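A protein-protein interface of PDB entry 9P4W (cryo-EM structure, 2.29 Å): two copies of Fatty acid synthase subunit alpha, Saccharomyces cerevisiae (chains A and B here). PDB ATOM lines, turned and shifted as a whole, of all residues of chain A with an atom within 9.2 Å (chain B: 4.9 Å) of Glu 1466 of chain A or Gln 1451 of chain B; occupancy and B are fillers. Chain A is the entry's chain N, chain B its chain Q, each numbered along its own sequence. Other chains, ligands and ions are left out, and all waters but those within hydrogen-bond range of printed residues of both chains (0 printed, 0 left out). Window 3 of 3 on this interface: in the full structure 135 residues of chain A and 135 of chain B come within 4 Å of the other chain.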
ATOM      1  N   ARG A1455     -24.757 -14.947  17.144  1.00  0.00           N
ATOM      2  CA  ARG A1455     -23.476 -14.993  16.478  1.00  0.00           C
ATOM      3  C   ARG A1455     -22.363 -15.228  17.488  1.00  0.00           C
ATOM      4  O   ARG A1455     -21.405 -15.924  17.199  1.00  0.00           O
ATOM      5  CB  ARG A1455     -23.232 -13.728  15.659  1.00  0.00           C
ATOM      6  CG  ARG A1455     -21.891 -13.690  14.964  1.00  0.00           C
ATOM      7  CD  ARG A1455     -21.916 -14.484  13.679  1.00  0.00           C
ATOM      8  NE  ARG A1455     -20.617 -14.444  13.030  1.00  0.00           N
ATOM      9  CZ  ARG A1455     -19.672 -15.356  13.207  1.00  0.00           C
ATOM     10  NH1 ARG A1455     -19.895 -16.389  14.004  1.00  0.00           N
ATOM     11  NH2 ARG A1455     -18.513 -15.240  12.580  1.00  0.00           N
ATOM     12  N   GLN A1458     -22.137 -18.912  18.043  1.00  0.00           N
ATOM     13  CA  GLN A1458     -21.431 -19.543  16.930  1.00  0.00           C
ATOM     14  C   GLN A1458     -19.935 -19.253  16.988  1.00  0.00           C
ATOM     15  O   GLN A1458     -19.113 -20.117  16.646  1.00  0.00           O
ATOM     16  CB  GLN A1458     -22.020 -19.074  15.602  1.00  0.00           C
ATOM     17  CG  GLN A1458     -23.430 -19.578  15.355  1.00  0.00           C
ATOM     18  CD  GLN A1458     -24.097 -18.902  14.178  1.00  0.00           C
ATOM     19  OE1 GLN A1458     -24.407 -17.714  14.225  1.00  0.00           O
ATOM     20  NE2 GLN A1458     -24.323 -19.660  13.113  1.00  0.00           N
ATOM     21  N   ILE A1459     -19.563 -18.052  17.432  1.00  0.00           N
ATOM     22  CA  ILE A1459     -18.154 -17.693  17.522  1.00  0.00           C
ATOM     23  C   ILE A1459     -17.445 -18.565  18.551  1.00  0.00           C
ATOM     24  O   ILE A1459     -16.333 -19.043  18.309  1.00  0.00           O
ATOM     25  CB  ILE A1459     -18.003 -16.198  17.850  1.00  0.00           C
ATOM     26  CG1 ILE A1459     -18.339 -15.352  16.623  1.00  0.00           C
ATOM     27  CG2 ILE A1459     -16.590 -15.895  18.329  1.00  0.00           C
ATOM     28  CD1 ILE A1459     -18.731 -13.930  16.947  1.00  0.00           C
ATOM     29  N   LYS A1460     -18.058 -18.769  19.719  1.00  0.00           N
ATOM     30  CA  LYS A1460     -17.402 -19.605  20.723  1.00  0.00           C
ATOM     31  C   LYS A1460     -17.261 -21.039  20.222  1.00  0.00           C
ATOM     32  O   LYS A1460     -16.263 -21.715  20.514  1.00  0.00           O
ATOM     33  CB  LYS A1460     -18.159 -19.573  22.053  1.00  0.00           C
ATOM     34  CG  LYS A1460     -19.577 -20.100  22.008  1.00  0.00           C
ATOM     35  CD  LYS A1460     -20.061 -20.492  23.398  1.00  0.00           C
ATOM     36  CE  LYS A1460     -21.525 -20.912  23.395  1.00  0.00           C
ATOM     37  NZ  LYS A1460     -21.883 -21.727  22.200  1.00  0.00           N
ATOM     38  N   ASP A1461     -18.249 -21.524  19.465  1.00  0.00           N
ATOM     39  CA  ASP A1461     -18.119 -22.855  18.874  1.00  0.00           C
ATOM     40  C   ASP A1461     -16.920 -22.921  17.933  1.00  0.00           C
ATOM     41  O   ASP A1461     -16.119 -23.870  17.978  1.00  0.00           O
ATOM     42  CB  ASP A1461     -19.404 -23.227  18.134  1.00  0.00           C
ATOM     43  CG  ASP A1461     -20.535 -23.582  19.075  1.00  0.00           C
ATOM     44  OD1 ASP A1461     -20.347 -23.460  20.303  1.00  0.00           O
ATOM     45  OD2 ASP A1461     -21.610 -23.985  18.588  1.00  0.00           O
ATOM     46  N   TRP A1462     -16.781 -21.917  17.063  1.00  0.00           N
ATOM     47  CA  TRP A1462     -15.620 -21.865  16.181  1.00  0.00           C
ATOM     48  C   TRP A1462     -14.332 -21.851  16.995  1.00  0.00           C
ATOM     49  O   TRP A1462     -13.356 -22.532  16.653  1.00  0.00           O
ATOM     50  CB  TRP A1462     -15.706 -20.628  15.283  1.00  0.00           C
ATOM     51  CG  TRP A1462     -14.534 -20.411  14.364  1.00  0.00           C
ATOM     52  CD1 TRP A1462     -14.469 -20.734  13.041  1.00  0.00           C
ATOM     53  CD2 TRP A1462     -13.274 -19.807  14.689  1.00  0.00           C
ATOM     54  NE1 TRP A1462     -13.248 -20.377  12.523  1.00  0.00           N
ATOM     55  CE2 TRP A1462     -12.496 -19.803  13.514  1.00  0.00           C
ATOM     56  CE3 TRP A1462     -12.728 -19.270  15.859  1.00  0.00           C
ATOM     57  CZ2 TRP A1462     -11.202 -19.291  13.477  1.00  0.00           C
ATOM     58  CZ3 TRP A1462     -11.441 -18.761  15.820  1.00  0.00           C
ATOM     59  CH2 TRP A1462     -10.693 -18.777  14.637  1.00  0.00           C
ATOM     60  N   VAL A1463     -14.324 -21.086  18.088  1.00  0.00           N
ATOM     61  CA  VAL A1463     -13.122 -20.953  18.907  1.00  0.00           C
ATOM     62  C   VAL A1463     -12.718 -22.302  19.483  1.00  0.00           C
ATOM     63  O   VAL A1463     -11.540 -22.673  19.463  1.00  0.00           O
ATOM     64  CB  VAL A1463     -13.343 -19.917  20.022  1.00  0.00           C
ATOM     65  CG1 VAL A1463     -12.226 -20.001  21.054  1.00  0.00           C
ATOM     66  CG2 VAL A1463     -13.410 -18.528  19.436  1.00  0.00           C
ATOM     67  N   GLU A1464     -13.681 -23.049  20.025  1.00  0.00           N
ATOM     68  CA  GLU A1464     -13.321 -24.316  20.656  1.00  0.00           C
ATOM     69  C   GLU A1464     -12.884 -25.344  19.616  1.00  0.00           C
ATOM     70  O   GLU A1464     -11.924 -26.095  19.844  1.00  0.00           O
ATOM     71  CB  GLU A1464     -14.474 -24.843  21.518  1.00  0.00           C
ATOM     72  CG  GLU A1464     -15.770 -25.154  20.792  1.00  0.00           C
ATOM     73  CD  GLU A1464     -15.778 -26.526  20.144  1.00  0.00           C
ATOM     74  OE1 GLU A1464     -14.819 -27.298  20.353  1.00  0.00           O
ATOM     75  OE2 GLU A1464     -16.753 -26.840  19.430  1.00  0.00           O
ATOM     76  N   ASN A1465     -13.549 -25.379  18.455  1.00  0.00           N
ATOM     77  CA  ASN A1465     -13.092 -26.283  17.399  1.00  0.00           C
ATOM     78  C   ASN A1465     -11.660 -25.965  16.988  1.00  0.00           C
ATOM     79  O   ASN A1465     -10.822 -26.870  16.846  1.00  0.00           O
ATOM     80  CB  ASN A1465     -14.020 -26.201  16.189  1.00  0.00           C
ATOM     81  CG  ASN A1465     -15.382 -26.797  16.456  1.00  0.00           C
ATOM     82  OD1 ASN A1465     -15.549 -27.615  17.358  1.00  0.00           O
ATOM     83  ND2 ASN A1465     -16.369 -26.394  15.665  1.00  0.00           N
ATOM     84  N   GLU A1466     -11.351 -24.683  16.804  1.00  0.00           N
ATOM     85  CA  GLU A1466     -10.018 -24.316  16.343  1.00  0.00           C
ATOM     86  C   GLU A1466      -8.977 -24.536  17.432  1.00  0.00           C
ATOM     87  O   GLU A1466      -7.822 -24.849  17.132  1.00  0.00           O
ATOM     88  CB  GLU A1466     -10.012 -22.868  15.865  1.00  0.00           C
ATOM     89  CG  GLU A1466     -11.035 -22.586  14.786  1.00  0.00           C
ATOM     90  CD  GLU A1466     -10.535 -22.916  13.397  1.00  0.00           C
ATOM     91  OE1 GLU A1466      -9.318 -22.782  13.147  1.00  0.00           O
ATOM     92  OE2 GLU A1466     -11.362 -23.317  12.551  1.00  0.00           O
ATOM     93  N   LEU A1467      -9.360 -24.379  18.701  1.00  0.00           N
ATOM     94  CA  LEU A1467      -8.437 -24.706  19.783  1.00  0.00           C
ATOM     95  C   LEU A1467      -8.128 -26.196  19.804  1.00  0.00           C
ATOM     96  O   LEU A1467      -6.982 -26.592  20.042  1.00  0.00           O
ATOM     97  CB  LEU A1467      -9.006 -24.259  21.131  1.00  0.00           C
ATOM     98  CG  LEU A1467      -8.547 -22.883  21.619  1.00  0.00           C
ATOM     99  CD1 LEU A1467      -9.423 -22.404  22.764  1.00  0.00           C
ATOM    100  CD2 LEU A1467      -7.083 -22.916  22.042  1.00  0.00           C
ATOM    101  N   GLU A1468      -9.131 -27.041  19.558  1.00  0.00           N
ATOM    102  CA  GLU A1468      -8.864 -28.475  19.476  1.00  0.00           C
ATOM    103  C   GLU A1468      -7.921 -28.788  18.316  1.00  0.00           C
ATOM    104  O   GLU A1468      -6.980 -29.583  18.459  1.00  0.00           O
ATOM    105  CB  GLU A1468     -10.181 -29.240  19.335  1.00  0.00           C
ATOM    106  CG  GLU A1468     -10.054 -30.631  18.732  1.00  0.00           C
ATOM    107  CD  GLU A1468     -10.403 -30.654  17.260  1.00  0.00           C
ATOM    108  OE1 GLU A1468     -11.549 -30.299  16.914  1.00  0.00           O
ATOM    109  OE2 GLU A1468      -9.529 -31.018  16.446  1.00  0.00           O
ATOM    110  N   ALA A1469      -8.149 -28.163  17.161  1.00  0.00           N
ATOM    111  CA  ALA A1469      -7.254 -28.367  16.026  1.00  0.00           C
ATOM    112  C   ALA A1469      -5.837 -27.878  16.306  1.00  0.00           C
ATOM    113  O   ALA A1469      -4.872 -28.538  15.900  1.00  0.00           O
ATOM    114  CB  ALA A1469      -7.808 -27.662  14.787  1.00  0.00           C
ATOM    115  N   LEU A1470      -5.687 -26.741  16.987  1.00  0.00           N
ATOM    116  CA  LEU A1470      -4.365 -26.254  17.368  1.00  0.00           C
ATOM    117  C   LEU A1470      -3.702 -27.181  18.376  1.00  0.00           C
ATOM    118  O   LEU A1470      -2.479 -27.350  18.360  1.00  0.00           O
ATOM    119  CB  LEU A1470      -4.480 -24.841  17.939  1.00  0.00           C
ATOM    120  CG  LEU A1470      -3.224 -24.263  18.592  1.00  0.00           C
ATOM    121  CD1 LEU A1470      -2.074 -24.211  17.597  1.00  0.00           C
ATOM    122  CD2 LEU A1470      -3.522 -22.883  19.157  1.00  0.00           C
ATOM    123  N   LEU A1486       2.848 -23.266  20.840  1.00  0.00           N
ATOM    124  CA  LEU A1486       1.481 -23.317  21.361  1.00  0.00           C
ATOM    125  C   LEU A1486       1.039 -21.934  21.857  1.00  0.00           C
ATOM    126  O   LEU A1486      -0.078 -21.548  21.630  1.00  0.00           O
ATOM    127  CB  LEU A1486       1.336 -24.358  22.466  1.00  0.00           C
ATOM    128  CG  LEU A1486       0.617 -25.633  22.035  1.00  0.00           C
ATOM    129  CD1 LEU A1486      -0.842 -25.350  21.724  1.00  0.00           C
ATOM    130  CD2 LEU A1486       1.303 -26.219  20.819  1.00  0.00           C
ATOM    131  N   ARG A1489       0.148 -19.742  19.010  1.00  0.00           N
ATOM    132  CA  ARG A1489      -1.111 -20.099  18.387  1.00  0.00           C
ATOM    133  C   ARG A1489      -2.356 -19.849  19.227  1.00  0.00           C
ATOM    134  O   ARG A1489      -3.395 -19.536  18.673  1.00  0.00           O
ATOM    135  CB  ARG A1489      -1.063 -21.534  17.961  1.00  0.00           C
ATOM    136  CG  ARG A1489      -0.144 -21.788  16.781  1.00  0.00           C
ATOM    137  CD  ARG A1489      -0.513 -20.907  15.599  1.00  0.00           C
ATOM    138  NE  ARG A1489      -1.956 -20.692  15.516  1.00  0.00           N
ATOM    139  CZ  ARG A1489      -2.828 -21.580  15.048  1.00  0.00           C
ATOM    140  NH1 ARG A1489      -2.422 -22.764  14.613  1.00  0.00           N
ATOM    141  NH2 ARG A1489      -4.117 -21.280  15.025  1.00  0.00           N
ATOM    142  N   THR A1490      -2.282 -20.011  20.535  1.00  0.00           N
ATOM    143  CA  THR A1490      -3.422 -19.689  21.365  1.00  0.00           C
ATOM    144  C   THR A1490      -3.662 -18.206  21.173  1.00  0.00           C
ATOM    145  O   THR A1490      -4.800 -17.762  20.983  1.00  0.00           O
ATOM    146  CB  THR A1490      -3.181 -20.051  22.843  1.00  0.00           C
ATOM    147  OG1 THR A1490      -4.349 -20.692  23.374  1.00  0.00           O
ATOM    148  CG2 THR A1490      -2.856 -18.821  23.682  1.00  0.00           C
ATOM    149  N   GLU A1492      -3.039 -16.373  18.637  1.00  0.00           N
ATOM    150  CA  GLU A1492      -3.693 -16.198  17.351  1.00  0.00           C
ATOM    151  C   GLU A1492      -5.174 -16.569  17.346  1.00  0.00           C
ATOM    152  O   GLU A1492      -5.995 -15.806  16.839  1.00  0.00           O
ATOM    153  CB  GLU A1492      -2.942 -17.038  16.309  1.00  0.00           C
ATOM    154  CG  GLU A1492      -3.825 -17.607  15.215  1.00  0.00           C
ATOM    155  CD  GLU A1492      -4.606 -16.536  14.482  1.00  0.00           C
ATOM    156  OE1 GLU A1492      -4.113 -15.393  14.385  1.00  0.00           O
ATOM    157  OE2 GLU A1492      -5.717 -16.836  14.003  1.00  0.00           O
ATOM    158  N   ILE A1493      -5.523 -17.724  17.885  1.00  0.00           N
ATOM    159  CA  ILE A1493      -6.904 -18.159  17.869  1.00  0.00           C
ATOM    160  C   ILE A1493      -7.785 -17.215  18.679  1.00  0.00           C
ATOM    161  O   ILE A1493      -8.889 -16.862  18.244  1.00  0.00           O
ATOM    162  CB  ILE A1493      -7.053 -19.585  18.398  1.00  0.00           C
ATOM    163  CG1 ILE A1493      -8.510 -20.015  18.355  1.00  0.00           C
ATOM    164  CG2 ILE A1493      -6.553 -19.712  19.824  1.00  0.00           C
ATOM    165  CD1 ILE A1493      -8.640 -21.514  18.352  1.00  0.00           C
ATOM    166  N   HIS A1494      -7.313 -16.769  19.836  1.00  0.00           N
ATOM    167  CA  HIS A1494      -8.186 -15.929  20.649  1.00  0.00           C
ATOM    168  C   HIS A1494      -8.334 -14.610  19.942  1.00  0.00           C
ATOM    169  O   HIS A1494      -9.390 -13.973  19.984  1.00  0.00           O
ATOM    170  CB  HIS A1494      -7.638 -15.782  22.055  1.00  0.00           C
ATOM    171  CG  HIS A1494      -7.438 -17.092  22.746  1.00  0.00           C
ATOM    172  ND1 HIS A1494      -6.279 -17.410  23.420  1.00  0.00           N
ATOM    173  CD2 HIS A1494      -8.239 -18.180  22.835  1.00  0.00           C
ATOM    174  CE1 HIS A1494      -6.383 -18.630  23.914  1.00  0.00           C
ATOM    175  NE2 HIS A1494      -7.561 -19.121  23.570  1.00  0.00           N
ATOM    176  N   GLU A1496      -8.403 -14.149  16.657  1.00  0.00           N
ATOM    177  CA  GLU A1496      -9.397 -14.286  15.593  1.00  0.00           C
ATOM    178  C   GLU A1496     -10.783 -14.340  16.174  1.00  0.00           C
ATOM    179  O   GLU A1496     -11.743 -13.862  15.564  1.00  0.00           O
ATOM    180  CB  GLU A1496      -9.147 -15.533  14.755  1.00  0.00           C
ATOM    181  N   ALA A1497     -10.903 -14.922  17.351  1.00  0.00           N
ATOM    182  CA  ALA A1497     -12.185 -14.925  18.000  1.00  0.00           C
ATOM    183  C   ALA A1497     -12.630 -13.493  18.265  1.00  0.00           C
ATOM    184  O   ALA A1497     -13.800 -13.134  18.062  1.00  0.00           O
ATOM    185  CB  ALA A1497     -12.075 -15.663  19.303  1.00  0.00           C
ATOM    186  N   GLN A1500     -13.768 -11.756  15.206  1.00  0.00           N
ATOM    187  CA  GLN A1500     -15.126 -12.104  14.828  1.00  0.00           C
ATOM    188  C   GLN A1500     -16.190 -11.496  15.728  1.00  0.00           C
ATOM    189  O   GLN A1500     -17.260 -11.139  15.256  1.00  0.00           O
ATOM    190  CB  GLN A1500     -15.267 -13.606  14.829  1.00  0.00           C
ATOM    191  CG  GLN A1500     -14.398 -14.293  13.794  1.00  0.00           C
ATOM    192  CD  GLN A1500     -14.350 -15.790  13.990  1.00  0.00           C
ATOM    193  OE1 GLN A1500     -15.090 -16.344  14.802  1.00  0.00           O
ATOM    194  NE2 GLN A1500     -13.476 -16.455  13.250  1.00  0.00           N
ATOM    195  N   TYR B1447      -5.704 -21.005   4.161  1.00  0.00           N
ATOM    196  CA  TYR B1447      -6.365 -21.050   5.462  1.00  0.00           C
ATOM    197  C   TYR B1447      -7.495 -20.029   5.543  1.00  0.00           C
ATOM    198  O   TYR B1447      -8.589 -20.330   6.042  1.00  0.00           O
ATOM    199  CB  TYR B1447      -5.318 -20.815   6.553  1.00  0.00           C
ATOM    200  CG  TYR B1447      -5.859 -20.461   7.918  1.00  0.00           C
ATOM    201  CD1 TYR B1447      -6.154 -19.147   8.254  1.00  0.00           C
ATOM    202  CD2 TYR B1447      -6.046 -21.439   8.882  1.00  0.00           C
ATOM    203  CE1 TYR B1447      -6.638 -18.822   9.504  1.00  0.00           C
ATOM    204  CE2 TYR B1447      -6.529 -21.125  10.134  1.00  0.00           C
ATOM    205  CZ  TYR B1447      -6.823 -19.815  10.440  1.00  0.00           C
ATOM    206  OH  TYR B1447      -7.304 -19.499  11.688  1.00  0.00           O
ATOM    207  N   ARG B1448      -7.259 -18.845   4.990  1.00  0.00           N
ATOM    208  CA  ARG B1448      -8.261 -17.794   5.040  1.00  0.00           C
ATOM    209  C   ARG B1448      -9.444 -18.176   4.180  1.00  0.00           C
ATOM    210  O   ARG B1448     -10.577 -17.958   4.573  1.00  0.00           O
ATOM    211  CB  ARG B1448      -7.652 -16.473   4.598  1.00  0.00           C
ATOM    212  CG  ARG B1448      -6.463 -16.007   5.421  1.00  0.00           C
ATOM    213  CD  ARG B1448      -6.236 -14.509   5.278  1.00  0.00           C
ATOM    214  NE  ARG B1448      -6.197 -14.072   3.885  1.00  0.00           N
ATOM    215  CZ  ARG B1448      -5.101 -14.009   3.134  1.00  0.00           C
ATOM    216  NH1 ARG B1448      -3.920 -14.359   3.616  1.00  0.00           N
ATOM    217  NH2 ARG B1448      -5.193 -13.595   1.884  1.00  0.00           N
ATOM    218  N   LYS B1449      -9.199 -18.779   3.026  1.00  0.00           N
ATOM    219  CA  LYS B1449     -10.287 -19.243   2.174  1.00  0.00           C
ATOM    220  C   LYS B1449     -11.090 -20.343   2.859  1.00  0.00           C
ATOM    221  O   LYS B1449     -12.323 -20.381   2.753  1.00  0.00           O
ATOM    222  CB  LYS B1449      -9.729 -19.737   0.838  1.00  0.00           C
ATOM    223  CG  LYS B1449     -10.785 -20.084  -0.203  1.00  0.00           C
ATOM    224  CD  LYS B1449     -11.714 -18.913  -0.488  1.00  0.00           C
ATOM    225  CE  LYS B1449     -12.664 -19.219  -1.631  1.00  0.00           C
ATOM    226  NZ  LYS B1449     -11.950 -19.499  -2.903  1.00  0.00           N
ATOM    227  N   ARG B1450     -10.406 -21.252   3.557  1.00  0.00           N
ATOM    228  CA  ARG B1450     -11.101 -22.302   4.298  1.00  0.00           C
ATOM    229  C   ARG B1450     -12.054 -21.697   5.322  1.00  0.00           C
ATOM    230  O   ARG B1450     -13.237 -22.070   5.399  1.00  0.00           O
ATOM    231  CB  ARG B1450     -10.076 -23.205   4.989  1.00  0.00           C
ATOM    232  CG  ARG B1450     -10.087 -24.661   4.542  1.00  0.00           C
ATOM    233  CD  ARG B1450      -8.672 -25.194   4.351  1.00  0.00           C
ATOM    234  NE  ARG B1450      -7.855 -25.037   5.551  1.00  0.00           N
ATOM    235  CZ  ARG B1450      -6.540 -24.853   5.557  1.00  0.00           C
ATOM    236  NH1 ARG B1450      -5.840 -24.817   4.434  1.00  0.00           N
ATOM    237  NH2 ARG B1450      -5.911 -24.703   6.719  1.00  0.00           N
ATOM    238  N   GLN B1451     -11.546 -20.761   6.125  1.00  0.00           N
ATOM    239  CA  GLN B1451     -12.397 -20.090   7.100  1.00  0.00           C
ATOM    240  C   GLN B1451     -13.569 -19.398   6.414  1.00  0.00           C
ATOM    241  O   GLN B1451     -14.687 -19.372   6.946  1.00  0.00           O
ATOM    242  CB  GLN B1451     -11.578 -19.082   7.903  1.00  0.00           C
ATOM    243  CG  GLN B1451     -10.413 -19.686   8.668  1.00  0.00           C
ATOM    244  CD  GLN B1451     -10.863 -20.571   9.812  1.00  0.00           C
ATOM    245  OE1 GLN B1451     -12.051 -20.654  10.120  1.00  0.00           O
ATOM    246  NE2 GLN B1451      -9.909 -21.236  10.453  1.00  0.00           N
ATOM    247  N   LEU B1452     -13.328 -18.832   5.230  1.00  0.00           N
ATOM    248  CA  LEU B1452     -14.393 -18.149   4.505  1.00  0.00           C
ATOM    249  C   LEU B1452     -15.503 -19.116   4.114  1.00  0.00           C
ATOM    250  O   LEU B1452     -16.690 -18.803   4.261  1.00  0.00           O
ATOM    251  CB  LEU B1452     -13.810 -17.458   3.270  1.00  0.00           C
ATOM    252  CG  LEU B1452     -14.684 -16.490   2.463  1.00  0.00           C
ATOM    253  CD1 LEU B1452     -15.401 -17.225   1.342  1.00  0.00           C
ATOM    254  CD2 LEU B1452     -15.680 -15.743   3.340  1.00  0.00           C
ATOM    255  N   VAL B1453     -15.141 -20.300   3.612  1.00  0.00           N
ATOM    256  CA  VAL B1453     -16.165 -21.288   3.261  1.00  0.00           C
ATOM    257  C   VAL B1453     -16.954 -21.697   4.498  1.00  0.00           C
ATOM    258  O   VAL B1453     -18.188 -21.824   4.454  1.00  0.00           O
ATOM    259  CB  VAL B1453     -15.553 -22.520   2.568  1.00  0.00           C
ATOM    260  CG1 VAL B1453     -16.623 -23.243   1.763  1.00  0.00           C
ATOM    261  CG2 VAL B1453     -14.409 -22.132   1.658  1.00  0.00           C
ATOM    262  N   THR B1454     -16.259 -21.933   5.612  1.00  0.00           N
ATOM    263  CA  THR B1454     -16.966 -22.301   6.837  1.00  0.00           C
ATOM    264  C   THR B1454     -17.980 -21.229   7.231  1.00  0.00           C
ATOM    265  O   THR B1454     -19.149 -21.533   7.528  1.00  0.00           O
ATOM    266  CB  THR B1454     -15.965 -22.531   7.968  1.00  0.00           C
ATOM    267  OG1 THR B1454     -14.812 -23.214   7.458  1.00  0.00           O
ATOM    268  CG2 THR B1454     -16.591 -23.362   9.072  1.00  0.00           C
ATOM    269  N   ARG B1455     -17.583 -19.968   7.217  1.00  0.00           N
ATOM    270  CA  ARG B1455     -18.503 -18.930   7.632  1.00  0.00           C
ATOM    271  C   ARG B1455     -19.660 -18.826   6.648  1.00  0.00           C
ATOM    272  O   ARG B1455     -20.792 -18.620   7.045  1.00  0.00           O
ATOM    273  CB  ARG B1455     -17.799 -17.582   7.792  1.00  0.00           C
ATOM    274  CG  ARG B1455     -18.078 -16.857   9.095  1.00  0.00           C
ATOM    275  CD  ARG B1455     -19.529 -16.993   9.500  1.00  0.00           C
ATOM    276  NE  ARG B1455     -20.151 -15.700   9.720  1.00  0.00           N
ATOM    277  CZ  ARG B1455     -21.422 -15.538  10.063  1.00  0.00           C
ATOM    278  NH1 ARG B1455     -22.203 -16.596  10.221  1.00  0.00           N
ATOM    279  NH2 ARG B1455     -21.913 -14.323  10.245  1.00  0.00           N
ATOM    280  N   TRP B1508     -11.685 -12.053   6.058  1.00  0.00           N
ATOM    281  CA  TRP B1508     -10.750 -13.093   5.644  1.00  0.00           C
ATOM    282  C   TRP B1508      -9.950 -12.761   4.391  1.00  0.00           C
ATOM    283  O   TRP B1508      -8.942 -13.430   4.137  1.00  0.00           O
ATOM    284  CB  TRP B1508     -11.490 -14.421   5.433  1.00  0.00           C
ATOM    285  CG  TRP B1508     -11.930 -15.033   6.725  1.00  0.00           C
ATOM    286  CD1 TRP B1508     -13.207 -15.303   7.116  1.00  0.00           C
ATOM    287  CD2 TRP B1508     -11.085 -15.434   7.809  1.00  0.00           C
ATOM    288  NE1 TRP B1508     -13.209 -15.853   8.374  1.00  0.00           N
ATOM    289  CE2 TRP B1508     -11.918 -15.942   8.822  1.00  0.00           C
ATOM    290  CE3 TRP B1508      -9.703 -15.413   8.020  1.00  0.00           C
ATOM    291  CZ2 TRP B1508     -11.416 -16.429  10.027  1.00  0.00           C
ATOM    292  CZ3 TRP B1508      -9.207 -15.896   9.214  1.00  0.00           C
ATOM    293  CH2 TRP B1508     -10.061 -16.395  10.203  1.00  0.00           C
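Among the printed residues, pairs that only touch across the chains: Gln 1500 of chain A with Trp 1508 of chain B (3.8 Å) and Glu 1492 of chain A with Tyr 1447 of chain B (3.9 Å).
The guanidinium group of Arg 1448 of chain B is in hydrogen-bond range of the backbone carbonyl oxygen of Trp 1508 of chain B (2.8 Å). The side-chain hydroxyl of Tyr 1447 of chain B lies within hydrogen-bond range of the side-chain amide nitrogen of Gln 1451 of chain B (3.4 Å). The side-chain carboxylate of Glu 1466 of chain A lies within hydrogen-bond range of the indole nitrogen of Trp 1462 of chain A (3.5 Å).
OE1 of Gln 1451 of chain B lies within hydrogen-bond range of NE1 of Trp 1462 of chain A (2.7 Å). The side-chain carboxylate of Glu 1466 of chain A is in hydrogen-bond range of the side-chain amide nitrogen of Gln 1451 of chain B, 3.2 Å away. The guanidinium group of Arg 1455 of chain A sits close to the guanidinium group of Arg 1455 of chain B (3.1 Å).
Arg 1455 of chain B touches its own counterpart, Arg 1455 of chain A.
Of the 10 printed residues of chain B, 4 touch a printed residue of chain A. Along chain B the printed residues that touch a printed residue of chain A span positions 1447 to 1508. Of the 23 printed residues of chain A, 5 touch a printed residue of chain B. Printed residues of chain A that touch a printed residue of chain B: Arg 1455, Trp 1462, Glu 1466, Glu 1492 and Gln 1500. Along chain A the printed residues that touch a printed residue of chain B span positions 1455 to 1500. Among the printed residues, no Asp or Glu carboxylate lies within 4 Å of a Lys or Arg side-chain nitrogen of the other chain.
Of chain B, only Gln 1451 comes within 4 Å of Glu 1466 of chain A. Of chain A, only Trp 1462 (2.7 Å) and Glu 1466 (3.2 Å) come within 4 Å of Gln 1451 of chain B. No residue of chain A comes within 4 Å of Thr 1454 of chain B. Of the printed residues of chain B, Glu 1492 of chain A touches Tyr 1447. Printed residues of chain B within 4 Å of Gln 1500 of chain A: Trp 1508. Of the printed residues of chain A, Trp 1508 of chain B touches Gln 1500. Val 1463 of chain A touches none of the printed residues of chain B. Arg 1450 of chain B touches none of the printed residues of chain A.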
